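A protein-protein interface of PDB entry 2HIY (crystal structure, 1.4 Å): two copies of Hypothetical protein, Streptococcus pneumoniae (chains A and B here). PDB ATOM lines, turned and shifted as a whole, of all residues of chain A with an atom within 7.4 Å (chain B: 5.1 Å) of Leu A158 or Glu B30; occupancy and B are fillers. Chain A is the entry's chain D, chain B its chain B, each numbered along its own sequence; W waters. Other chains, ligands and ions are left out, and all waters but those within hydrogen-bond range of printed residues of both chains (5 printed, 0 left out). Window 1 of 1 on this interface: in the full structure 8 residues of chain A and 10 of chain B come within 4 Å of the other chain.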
ATOM      1  N   ARG A  12      28.212 -13.973 -20.559  1.00  0.00           N
ATOM      2  CA  ARG A  12      27.846 -13.827 -19.157  1.00  0.00           C
ATOM      3  C   ARG A  12      27.988 -15.149 -18.430  1.00  0.00           C
ATOM      4  O   ARG A  12      27.963 -16.229 -19.052  1.00  0.00           O
ATOM      5  CB  ARG A  12      26.383 -13.372 -19.055  1.00  0.00           C
ATOM      6  CG  ARG A  12      25.408 -14.420 -19.572  1.00  0.00           C
ATOM      7  CD  ARG A  12      24.087 -14.585 -18.799  1.00  0.00           C
ATOM      8  NE  ARG A  12      24.099 -14.138 -17.414  1.00  0.00           N
ATOM      9  CZ  ARG A  12      24.081 -14.929 -16.337  1.00  0.00           C
ATOM     10  NH1 ARG A  12      24.069 -14.369 -15.135  1.00  0.00           N
ATOM     11  NH2 ARG A  12      24.064 -16.243 -16.448  1.00  0.00           N
ATOM     12  N   ALA A 152      14.963   0.117  -9.350  1.00  0.00           N
ATOM     13  CA  ALA A 152      14.444  -0.988 -10.152  1.00  0.00           C
ATOM     14  C   ALA A 152      15.578  -1.880 -10.614  1.00  0.00           C
ATOM     15  O   ALA A 152      15.401  -3.105 -10.721  1.00  0.00           O
ATOM     16  CB  ALA A 152      13.695  -0.430 -11.344  1.00  0.00           C
ATOM     17  N   TYR A 153      16.732  -1.307 -10.937  1.00  0.00           N
ATOM     18  CA  TYR A 153      17.884  -2.112 -11.327  1.00  0.00           C
ATOM     19  C   TYR A 153      18.172  -3.184 -10.276  1.00  0.00           C
ATOM     20  O   TYR A 153      18.302  -4.387 -10.608  1.00  0.00           O
ATOM     21  CB  TYR A 153      19.107  -1.204 -11.515  1.00  0.00           C
ATOM     22  CG  TYR A 153      20.312  -1.915 -12.063  1.00  0.00           C
ATOM     23  CD1 TYR A 153      20.471  -2.045 -13.435  1.00  0.00           C
ATOM     24  CD2 TYR A 153      21.303  -2.439 -11.227  1.00  0.00           C
ATOM     25  CE1 TYR A 153      21.565  -2.732 -13.985  1.00  0.00           C
ATOM     26  CE2 TYR A 153      22.406  -3.139 -11.760  1.00  0.00           C
ATOM     27  CZ  TYR A 153      22.530  -3.252 -13.130  1.00  0.00           C
ATOM     28  OH  TYR A 153      23.638  -3.921 -13.621  1.00  0.00           O
ATOM     29  N   HIS A 154      18.269  -2.767  -9.028  1.00  0.00           N
ATOM     30  CA  HIS A 154      18.538  -3.710  -7.957  1.00  0.00           C
ATOM     31  C   HIS A 154      17.375  -4.639  -7.671  1.00  0.00           C
ATOM     32  O   HIS A 154      17.579  -5.867  -7.512  1.00  0.00           O
ATOM     33  CB  HIS A 154      18.894  -2.950  -6.689  1.00  0.00           C
ATOM     34  CG  HIS A 154      19.055  -3.843  -5.513  1.00  0.00           C
ATOM     35  ND1 HIS A 154      20.096  -4.752  -5.433  1.00  0.00           N
ATOM     36  CD2 HIS A 154      18.299  -4.008  -4.406  1.00  0.00           C
ATOM     37  CE1 HIS A 154      19.967  -5.433  -4.303  1.00  0.00           C
ATOM     38  NE2 HIS A 154      18.900  -4.995  -3.656  1.00  0.00           N
ATOM     39  N   LYS A 155      16.171  -4.063  -7.530  1.00  0.00           N
ATOM     40  CA  LYS A 155      15.035  -4.848  -7.039  1.00  0.00           C
ATOM     41  C   LYS A 155      14.485  -5.812  -8.036  1.00  0.00           C
ATOM     42  O   LYS A 155      13.918  -6.838  -7.607  1.00  0.00           O
ATOM     43  CB  LYS A 155      13.907  -3.936  -6.601  1.00  0.00           C
ATOM     44  CG  LYS A 155      14.287  -3.154  -5.346  1.00  0.00           C
ATOM     45  CD  LYS A 155      13.211  -2.149  -4.983  1.00  0.00           C
ATOM     46  CE  LYS A 155      11.907  -2.835  -4.646  1.00  0.00           C
ATOM     47  NZ  LYS A 155      10.904  -1.815  -4.210  1.00  0.00           N
ATOM     48  N   TYR A 156      14.580  -5.506  -9.337  1.00  0.00           N
ATOM     49  CA  TYR A 156      13.802  -6.251 -10.310  1.00  0.00           C
ATOM     50  C   TYR A 156      14.549  -6.986 -11.375  1.00  0.00           C
ATOM     51  O   TYR A 156      13.946  -7.832 -12.013  1.00  0.00           O
ATOM     52  CB  TYR A 156      12.743  -5.369 -11.007  1.00  0.00           C
ATOM     53  CG  TYR A 156      11.869  -4.573 -10.077  1.00  0.00           C
ATOM     54  CD1 TYR A 156      11.245  -5.165  -8.978  1.00  0.00           C
ATOM     55  CD2 TYR A 156      11.684  -3.211 -10.285  1.00  0.00           C
ATOM     56  CE1 TYR A 156      10.435  -4.407  -8.109  1.00  0.00           C
ATOM     57  CE2 TYR A 156      10.882  -2.456  -9.430  1.00  0.00           C
ATOM     58  CZ  TYR A 156      10.277  -3.062  -8.347  1.00  0.00           C
ATOM     59  OH  TYR A 156       9.490  -2.316  -7.492  1.00  0.00           O
ATOM     60  N   LEU A 157      15.836  -6.727 -11.592  1.00  0.00           N
ATOM     61  CA  LEU A 157      16.474  -7.372 -12.743  1.00  0.00           C
ATOM     62  C   LEU A 157      16.612  -8.890 -12.657  1.00  0.00           C
ATOM     63  O   LEU A 157      16.672  -9.575 -13.683  1.00  0.00           O
ATOM     64  CB  LEU A 157      17.805  -6.727 -13.104  1.00  0.00           C
ATOM     65  CG  LEU A 157      17.693  -5.448 -13.935  1.00  0.00           C
ATOM     66  CD1 LEU A 157      19.085  -4.967 -14.268  1.00  0.00           C
ATOM     67  CD2 LEU A 157      16.822  -5.618 -15.205  1.00  0.00           C
ATOM     68  N   LEU A 158      16.680  -9.437 -11.447  1.00  0.00           N
ATOM     69  CA  LEU A 158      16.673 -10.910 -11.329  1.00  0.00           C
ATOM     70  C   LEU A 158      15.315 -11.523 -11.619  1.00  0.00           C
ATOM     71  O   LEU A 158      15.194 -12.737 -11.794  1.00  0.00           O
ATOM     72  CB  LEU A 158      17.134 -11.370  -9.957  1.00  0.00           C
ATOM     73  CG  LEU A 158      18.627 -11.251  -9.688  1.00  0.00           C
ATOM     74  CD1 LEU A 158      18.852 -11.572  -8.210  1.00  0.00           C
ATOM     75  CD2 LEU A 158      19.479 -12.164 -10.562  1.00  0.00           C
ATOM     76  N   LYS A 159      14.276 -10.694 -11.640  1.00  0.00           N
ATOM     77  CA  LYS A 159      12.925 -11.157 -11.931  1.00  0.00           C
ATOM     78  C   LYS A 159      12.589 -11.235 -13.425  1.00  0.00           C
ATOM     79  O   LYS A 159      11.539 -11.777 -13.775  1.00  0.00           O
ATOM     80  CB  LYS A 159      11.900 -10.267 -11.225  1.00  0.00           C
ATOM     81  CG  LYS A 159      12.052 -10.240  -9.704  1.00  0.00           C
ATOM     82  CD  LYS A 159      11.056  -9.261  -9.102  1.00  0.00           C
ATOM     83  CE  LYS A 159      11.282  -9.005  -7.604  1.00  0.00           C
ATOM     84  NZ  LYS A 159      10.962 -10.187  -6.771  1.00  0.00           N
ATOM     85  N   VAL A 160      13.432 -10.680 -14.299  1.00  0.00           N
ATOM     86  CA  VAL A 160      13.049 -10.560 -15.723  1.00  0.00           C
ATOM     87  C   VAL A 160      13.497 -11.781 -16.528  1.00  0.00           C
ATOM     88  O   VAL A 160      14.556 -12.358 -16.268  1.00  0.00           O
ATOM     89  CB  VAL A 160      13.599  -9.252 -16.381  1.00  0.00           C
ATOM     90  CG1 VAL A 160      13.068  -7.977 -15.646  1.00  0.00           C
ATOM     91  CG2 VAL A 160      15.126  -9.275 -16.501  1.00  0.00           C
ATOM     92  N   PRO A 161      12.692 -12.203 -17.505  1.00  0.00           N
ATOM     93  CA  PRO A 161      13.051 -13.331 -18.343  1.00  0.00           C
ATOM     94  C   PRO A 161      14.315 -13.104 -19.171  1.00  0.00           C
ATOM     95  O   PRO A 161      14.966 -14.075 -19.519  1.00  0.00           O
ATOM     96  CB  PRO A 161      11.802 -13.517 -19.236  1.00  0.00           C
ATOM     97  CG  PRO A 161      10.708 -12.878 -18.493  1.00  0.00           C
ATOM     98  CD  PRO A 161      11.316 -11.730 -17.770  1.00  0.00           C
ATOM     99  N   TYR A 163      17.161 -11.788 -18.282  1.00  0.00           N
ATOM    100  CA  TYR A 163      18.383 -11.624 -17.548  1.00  0.00           C
ATOM    101  C   TYR A 163      19.577 -12.431 -18.044  1.00  0.00           C
ATOM    102  O   TYR A 163      20.698 -11.892 -18.126  1.00  0.00           O
ATOM    103  CB  TYR A 163      18.122 -11.959 -16.077  1.00  0.00           C
ATOM    104  CG  TYR A 163      19.295 -11.678 -15.185  1.00  0.00           C
ATOM    105  CD1 TYR A 163      19.572 -10.373 -14.793  1.00  0.00           C
ATOM    106  CD2 TYR A 163      20.158 -12.703 -14.758  1.00  0.00           C
ATOM    107  CE1 TYR A 163      20.663 -10.080 -13.990  1.00  0.00           C
ATOM    108  CE2 TYR A 163      21.256 -12.410 -13.920  1.00  0.00           C
ATOM    109  CZ  TYR A 163      21.481 -11.083 -13.559  1.00  0.00           C
ATOM    110  OH  TYR A 163      22.549 -10.752 -12.741  1.00  0.00           O
ATOM    111  N   GLU B  26       7.679 -15.342 -10.074  1.00  0.00           N
ATOM    112  CA  GLU B  26       8.840 -14.462  -9.916  1.00  0.00           C
ATOM    113  C   GLU B  26       9.982 -15.207  -9.245  1.00  0.00           C
ATOM    114  O   GLU B  26      11.102 -15.145  -9.716  1.00  0.00           O
ATOM    115  CB  GLU B  26       8.529 -13.220  -9.082  1.00  0.00           C
ATOM    116  CG  GLU B  26       7.610 -12.243  -9.739  1.00  0.00           C
ATOM    117  CD  GLU B  26       7.383 -10.969  -8.924  1.00  0.00           C
ATOM    118  OE1 GLU B  26       8.016 -10.785  -7.847  1.00  0.00           O
ATOM    119  OE2 GLU B  26       6.565 -10.143  -9.399  1.00  0.00           O
ATOM    120  N   LEU B  27       9.685 -15.932  -8.159  1.00  0.00           N
ATOM    121  CA  LEU B  27      10.720 -16.637  -7.464  1.00  0.00           C
ATOM    122  C   LEU B  27      11.348 -17.695  -8.354  1.00  0.00           C
ATOM    123  O   LEU B  27      12.569 -17.863  -8.343  1.00  0.00           O
ATOM    124  CB  LEU B  27      10.177 -17.254  -6.176  1.00  0.00           C
ATOM    125  CG  LEU B  27      11.184 -18.076  -5.372  1.00  0.00           C
ATOM    126  CD1 LEU B  27      12.397 -17.253  -4.924  1.00  0.00           C
ATOM    127  CD2 LEU B  27      10.484 -18.684  -4.165  1.00  0.00           C
ATOM    128  N   ARG B  28      10.531 -18.431  -9.112  1.00  0.00           N
ATOM    129  CA  ARG B  28      11.111 -19.431  -9.994  1.00  0.00           C
ATOM    130  C   ARG B  28      12.053 -18.754 -10.996  1.00  0.00           C
ATOM    131  O   ARG B  28      13.116 -19.286 -11.315  1.00  0.00           O
ATOM    132  CB  ARG B  28      10.029 -20.206 -10.741  1.00  0.00           C
ATOM    133  CG  ARG B  28       9.204 -21.106  -9.809  1.00  0.00           C
ATOM    134  CD  ARG B  28       8.392 -22.137 -10.595  1.00  0.00           C
ATOM    135  NE  ARG B  28       7.550 -21.504 -11.598  1.00  0.00           N
ATOM    136  CZ  ARG B  28       6.301 -21.088 -11.427  1.00  0.00           C
ATOM    137  NH1 ARG B  28       5.651 -21.279 -10.293  1.00  0.00           N
ATOM    138  NH2 ARG B  28       5.660 -20.515 -12.431  1.00  0.00           N
ATOM    139  N   GLN B  29      11.630 -17.618 -11.542  1.00  0.00           N
ATOM    140  CA  GLN B  29      12.486 -16.898 -12.474  1.00  0.00           C
ATOM    141  C   GLN B  29      13.792 -16.415 -11.819  1.00  0.00           C
ATOM    142  O   GLN B  29      14.876 -16.486 -12.449  1.00  0.00           O
ATOM    143  CB  GLN B  29      11.711 -15.731 -13.113  1.00  0.00           C
ATOM    144  CG  GLN B  29      12.576 -14.931 -14.128  1.00  0.00           C
ATOM    145  CD  GLN B  29      12.891 -15.772 -15.344  1.00  0.00           C
ATOM    146  OE1 GLN B  29      13.992 -16.321 -15.495  1.00  0.00           O
ATOM    147  NE2 GLN B  29      11.915 -15.903 -16.209  1.00  0.00           N
ATOM    148  N   GLU B  30      13.697 -15.891 -10.595  1.00  0.00           N
ATOM    149  CA  GLU B  30      14.872 -15.431  -9.884  1.00  0.00           C
ATOM    150  C   GLU B  30      15.864 -16.568  -9.659  1.00  0.00           C
ATOM    151  O   GLU B  30      17.064 -16.432  -9.912  1.00  0.00           O
ATOM    152  CB  GLU B  30      14.478 -14.803  -8.559  1.00  0.00           C
ATOM    153  CG  GLU B  30      13.732 -13.467  -8.757  1.00  0.00           C
ATOM    154  CD  GLU B  30      13.026 -13.001  -7.489  1.00  0.00           C
ATOM    155  OE1 GLU B  30      12.267 -13.784  -6.902  1.00  0.00           O
ATOM    156  OE2 GLU B  30      13.224 -11.847  -7.068  1.00  0.00           O
ATOM    157  N   LEU B  31      15.365 -17.693  -9.159  1.00  0.00           N
ATOM    158  CA  LEU B  31      16.250 -18.829  -8.934  1.00  0.00           C
ATOM    159  C   LEU B  31      16.872 -19.385 -10.224  1.00  0.00           C
ATOM    160  O   LEU B  31      18.052 -19.751 -10.232  1.00  0.00           O
ATOM    161  CB  LEU B  31      15.509 -19.931  -8.184  1.00  0.00           C
ATOM    162  CG  LEU B  31      15.038 -19.517  -6.788  1.00  0.00           C
ATOM    163  CD1 LEU B  31      14.358 -20.704  -6.102  1.00  0.00           C
ATOM    164  CD2 LEU B  31      16.167 -19.006  -5.905  1.00  0.00           C
ATOM    165  N   THR B  32      16.106 -19.369 -11.316  1.00  0.00           N
ATOM    166  CA  THR B  32      16.641 -19.715 -12.644  1.00  0.00           C
ATOM    167  C   THR B  32      17.749 -18.731 -13.010  1.00  0.00           C
ATOM    168  O   THR B  32      18.807 -19.130 -13.513  1.00  0.00           O
ATOM    169  CB  THR B  32      15.498 -19.685 -13.687  1.00  0.00           C
ATOM    170  OG1 THR B  32      14.524 -20.674 -13.310  1.00  0.00           O
ATOM    171  CG2 THR B  32      15.983 -20.010 -15.090  1.00  0.00           C
ATOM    172  N   ASN B  33      17.522 -17.447 -12.744  1.00  0.00           N
ATOM    173  CA  ASN B  33      18.542 -16.443 -13.050  1.00  0.00           C
ATOM    174  C   ASN B  33      19.795 -16.531 -12.188  1.00  0.00           C
ATOM    175  O   ASN B  33      20.863 -16.038 -12.566  1.00  0.00           O
ATOM    176  CB  ASN B  33      17.932 -15.036 -13.043  1.00  0.00           C
ATOM    177  CG  ASN B  33      17.032 -14.797 -14.236  1.00  0.00           C
ATOM    178  OD1 ASN B  33      17.179 -15.437 -15.284  1.00  0.00           O
ATOM    179  ND2 ASN B  33      16.097 -13.859 -14.097  1.00  0.00           N
ATOM    180  N   LEU B  34      19.663 -17.156 -11.032  1.00  0.00           N
ATOM    181  CA  LEU B  34      20.829 -17.441 -10.188  1.00  0.00           C
ATOM    182  C   LEU B  34      21.562 -18.693 -10.626  1.00  0.00           C
ATOM    183  O   LEU B  34      22.573 -19.070 -10.004  1.00  0.00           O
ATOM    184  CB  LEU B  34      20.393 -17.637  -8.731  1.00  0.00           C
ATOM    185  CG  LEU B  34      19.870 -16.426  -7.975  1.00  0.00           C
ATOM    186  CD1 LEU B  34      19.579 -16.833  -6.533  1.00  0.00           C
ATOM    187  CD2 LEU B  34      20.825 -15.257  -8.037  1.00  0.00           C
ATOM    188  N   PHE B  66      20.762 -14.570  -1.203  1.00  0.00           N
ATOM    189  CA  PHE B  66      19.634 -14.130  -2.020  1.00  0.00           C
ATOM    190  C   PHE B  66      18.443 -13.679  -1.157  1.00  0.00           C
ATOM    191  O   PHE B  66      17.912 -12.576  -1.343  1.00  0.00           O
ATOM    192  CB  PHE B  66      19.209 -15.241  -2.984  1.00  0.00           C
ATOM    193  CG  PHE B  66      17.931 -14.942  -3.715  1.00  0.00           C
ATOM    194  CD1 PHE B  66      17.905 -13.996  -4.742  1.00  0.00           C
ATOM    195  CD2 PHE B  66      16.754 -15.594  -3.362  1.00  0.00           C
ATOM    196  CE1 PHE B  66      16.699 -13.700  -5.404  1.00  0.00           C
ATOM    197  CE2 PHE B  66      15.545 -15.315  -4.024  1.00  0.00           C
ATOM    198  CZ  PHE B  66      15.527 -14.379  -5.030  1.00  0.00           C
ATOM    199  N   HIS B  70      16.700  -9.996  -1.075  1.00  0.00           N
ATOM    200  CA  HIS B  70      15.462  -9.876  -1.862  1.00  0.00           C
ATOM    201  C   HIS B  70      14.163 -10.293  -1.169  1.00  0.00           C
ATOM    202  O   HIS B  70      13.080  -9.862  -1.582  1.00  0.00           O
ATOM    203  CB  HIS B  70      15.642 -10.635  -3.174  1.00  0.00           C
ATOM    204  CG  HIS B  70      16.679 -10.003  -4.041  1.00  0.00           C
ATOM    205  ND1 HIS B  70      16.456  -8.801  -4.691  1.00  0.00           N
ATOM    206  CD2 HIS B  70      17.962 -10.347  -4.297  1.00  0.00           C
ATOM    207  CE1 HIS B  70      17.557  -8.461  -5.337  1.00  0.00           C
ATOM    208  NE2 HIS B  70      18.482  -9.382  -5.119  1.00  0.00           N
ATOM    209  N   TYR B  71      14.259 -11.139  -0.143  1.00  0.00           N
ATOM    210  CA  TYR B  71      13.068 -11.564   0.637  1.00  0.00           C
ATOM    211  C   TYR B  71      13.509 -11.671   2.076  1.00  0.00           C
ATOM    212  O   TYR B  71      13.570 -12.790   2.600  1.00  0.00           O
ATOM    213  CB  TYR B  71      12.550 -12.930   0.152  1.00  0.00           C
ATOM    214  CG  TYR B  71      12.029 -12.902  -1.276  1.00  0.00           C
ATOM    215  CD1 TYR B  71      10.763 -12.386  -1.567  1.00  0.00           C
ATOM    216  CD2 TYR B  71      12.800 -13.399  -2.333  1.00  0.00           C
ATOM    217  CE1 TYR B  71      10.277 -12.355  -2.870  1.00  0.00           C
ATOM    218  CE2 TYR B  71      12.307 -13.386  -3.654  1.00  0.00           C
ATOM    219  CZ  TYR B  71      11.057 -12.887  -3.899  1.00  0.00           C
ATOM    220  OH  TYR B  71      10.540 -12.839  -5.175  1.00  0.00           O
HETATM  221  O   HOH W   1      22.458 -17.542 -14.224  1.00  0.00           O
HETATM  222  O   HOH W   2      23.276 -15.041 -12.278  1.00  0.00           O
HETATM  223  O   HOH W   3      14.005  -7.443  -4.922  1.00  0.00           O
HETATM  224  O   HOH W   4      16.916 -15.186 -17.931  1.00  0.00           O
HETATM  225  O   HOH W   5      11.961  -9.099  -4.143  1.00  0.00           O
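No position is printed for both chains. Of the 13 pairs that touch across the chains among the printed residues, none has its exchanged pair printed and touching as well.
Water W2 lies within hydrogen-bond range of the backbone carbonyl oxygen of Asn B33 (2.6 Å) and the guanidinium group of Arg A12 (3.0 Å). Water W4 lies within hydrogen-bond range of OD1 of Asn B33, O of Pro A161 and N of Tyr A163. Water W1 lies within hydrogen-bond range of O of Asn B33 (2.7 Å) and NH2 of Arg A12 (3.0 Å). Water W3 lies within hydrogen-bond range of the backbone carbonyl oxygen (O) of Lys A155 (2.8 Å) and a ring nitrogen (ND1) of His B70 (2.8 Å). Water W5 bridges O of His B70 (2.9 Å) and NZ of Lys A159 (3.0 Å).
Hydrophobic or aromatic side chains of chain A within 4 Å of the printed part of chain B: Leu A158, Pro A161 and Tyr A163. Among the printed residues, Asp or Glu carboxylates within 4 Å of a Lys or Arg side-chain nitrogen of the other chain: Lys A159 with Glu B26 (3.2 Å) and Lys A159 with Glu B30 (2.8 Å).
OE1 of Gln B29 lies close to OD1 of Asn B33 (3.3 Å). The side-chain carboxylate of Glu B30 is in hydrogen-bond range of the side-chain hydroxyl of Tyr B71, 2.6 Å away.
His A154 touches His B70. O of Leu A158 touches O of Gln B29 (3.8 Å). Glu B30 touches Leu A158 (CA to O, 3.3 Å). CD1 of Leu A158 touches NE2 of His B70, 3.8 Å away. Gln B29 touches Lys A159 (CG to O, 3.3 Å). Val A160 touches Gln B29. Pro A161 touches Gln B29. Asn B33 touches Tyr A163.
The side-chain amino group of Lys A159 is in salt-bridge range of the side-chain carboxylate of Glu B26 (3.2 Å). O of Leu A158 is in hydrogen-bond range of ND2 of Asn B33 (2.7 Å). The side-chain amino group of Lys A159 is in salt-bridge range of the side-chain carboxylate of Glu B30 (2.8 Å). OH of Tyr B71 is in hydrogen-bond range of NZ of Lys A159. O of Val A160 sits at hydrogen-bond distance from ND2 of Asn B33, 3.1 Å away.
Leu A158 touches four residues of chain B. Printed residues of chain B within 4 Å of Lys A159: Glu B26 (3.2 Å), Gln B29 (3.3 Å), Glu B30 (2.8 Å) and Tyr B71 (3.1 Å). Of chain A, only Leu A158 (3.3 Å) and Lys A159 (2.8 Å) come within 4 Å of Glu B30. Of the printed residues of chain A, Asn B33 touches Leu A158 (2.7 Å), Val A160 (3.1 Å) and Tyr A163 (3.4 Å). The nearest residue of chain A that does not touch Glu B30 is Lys A155 (5.1 Å).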
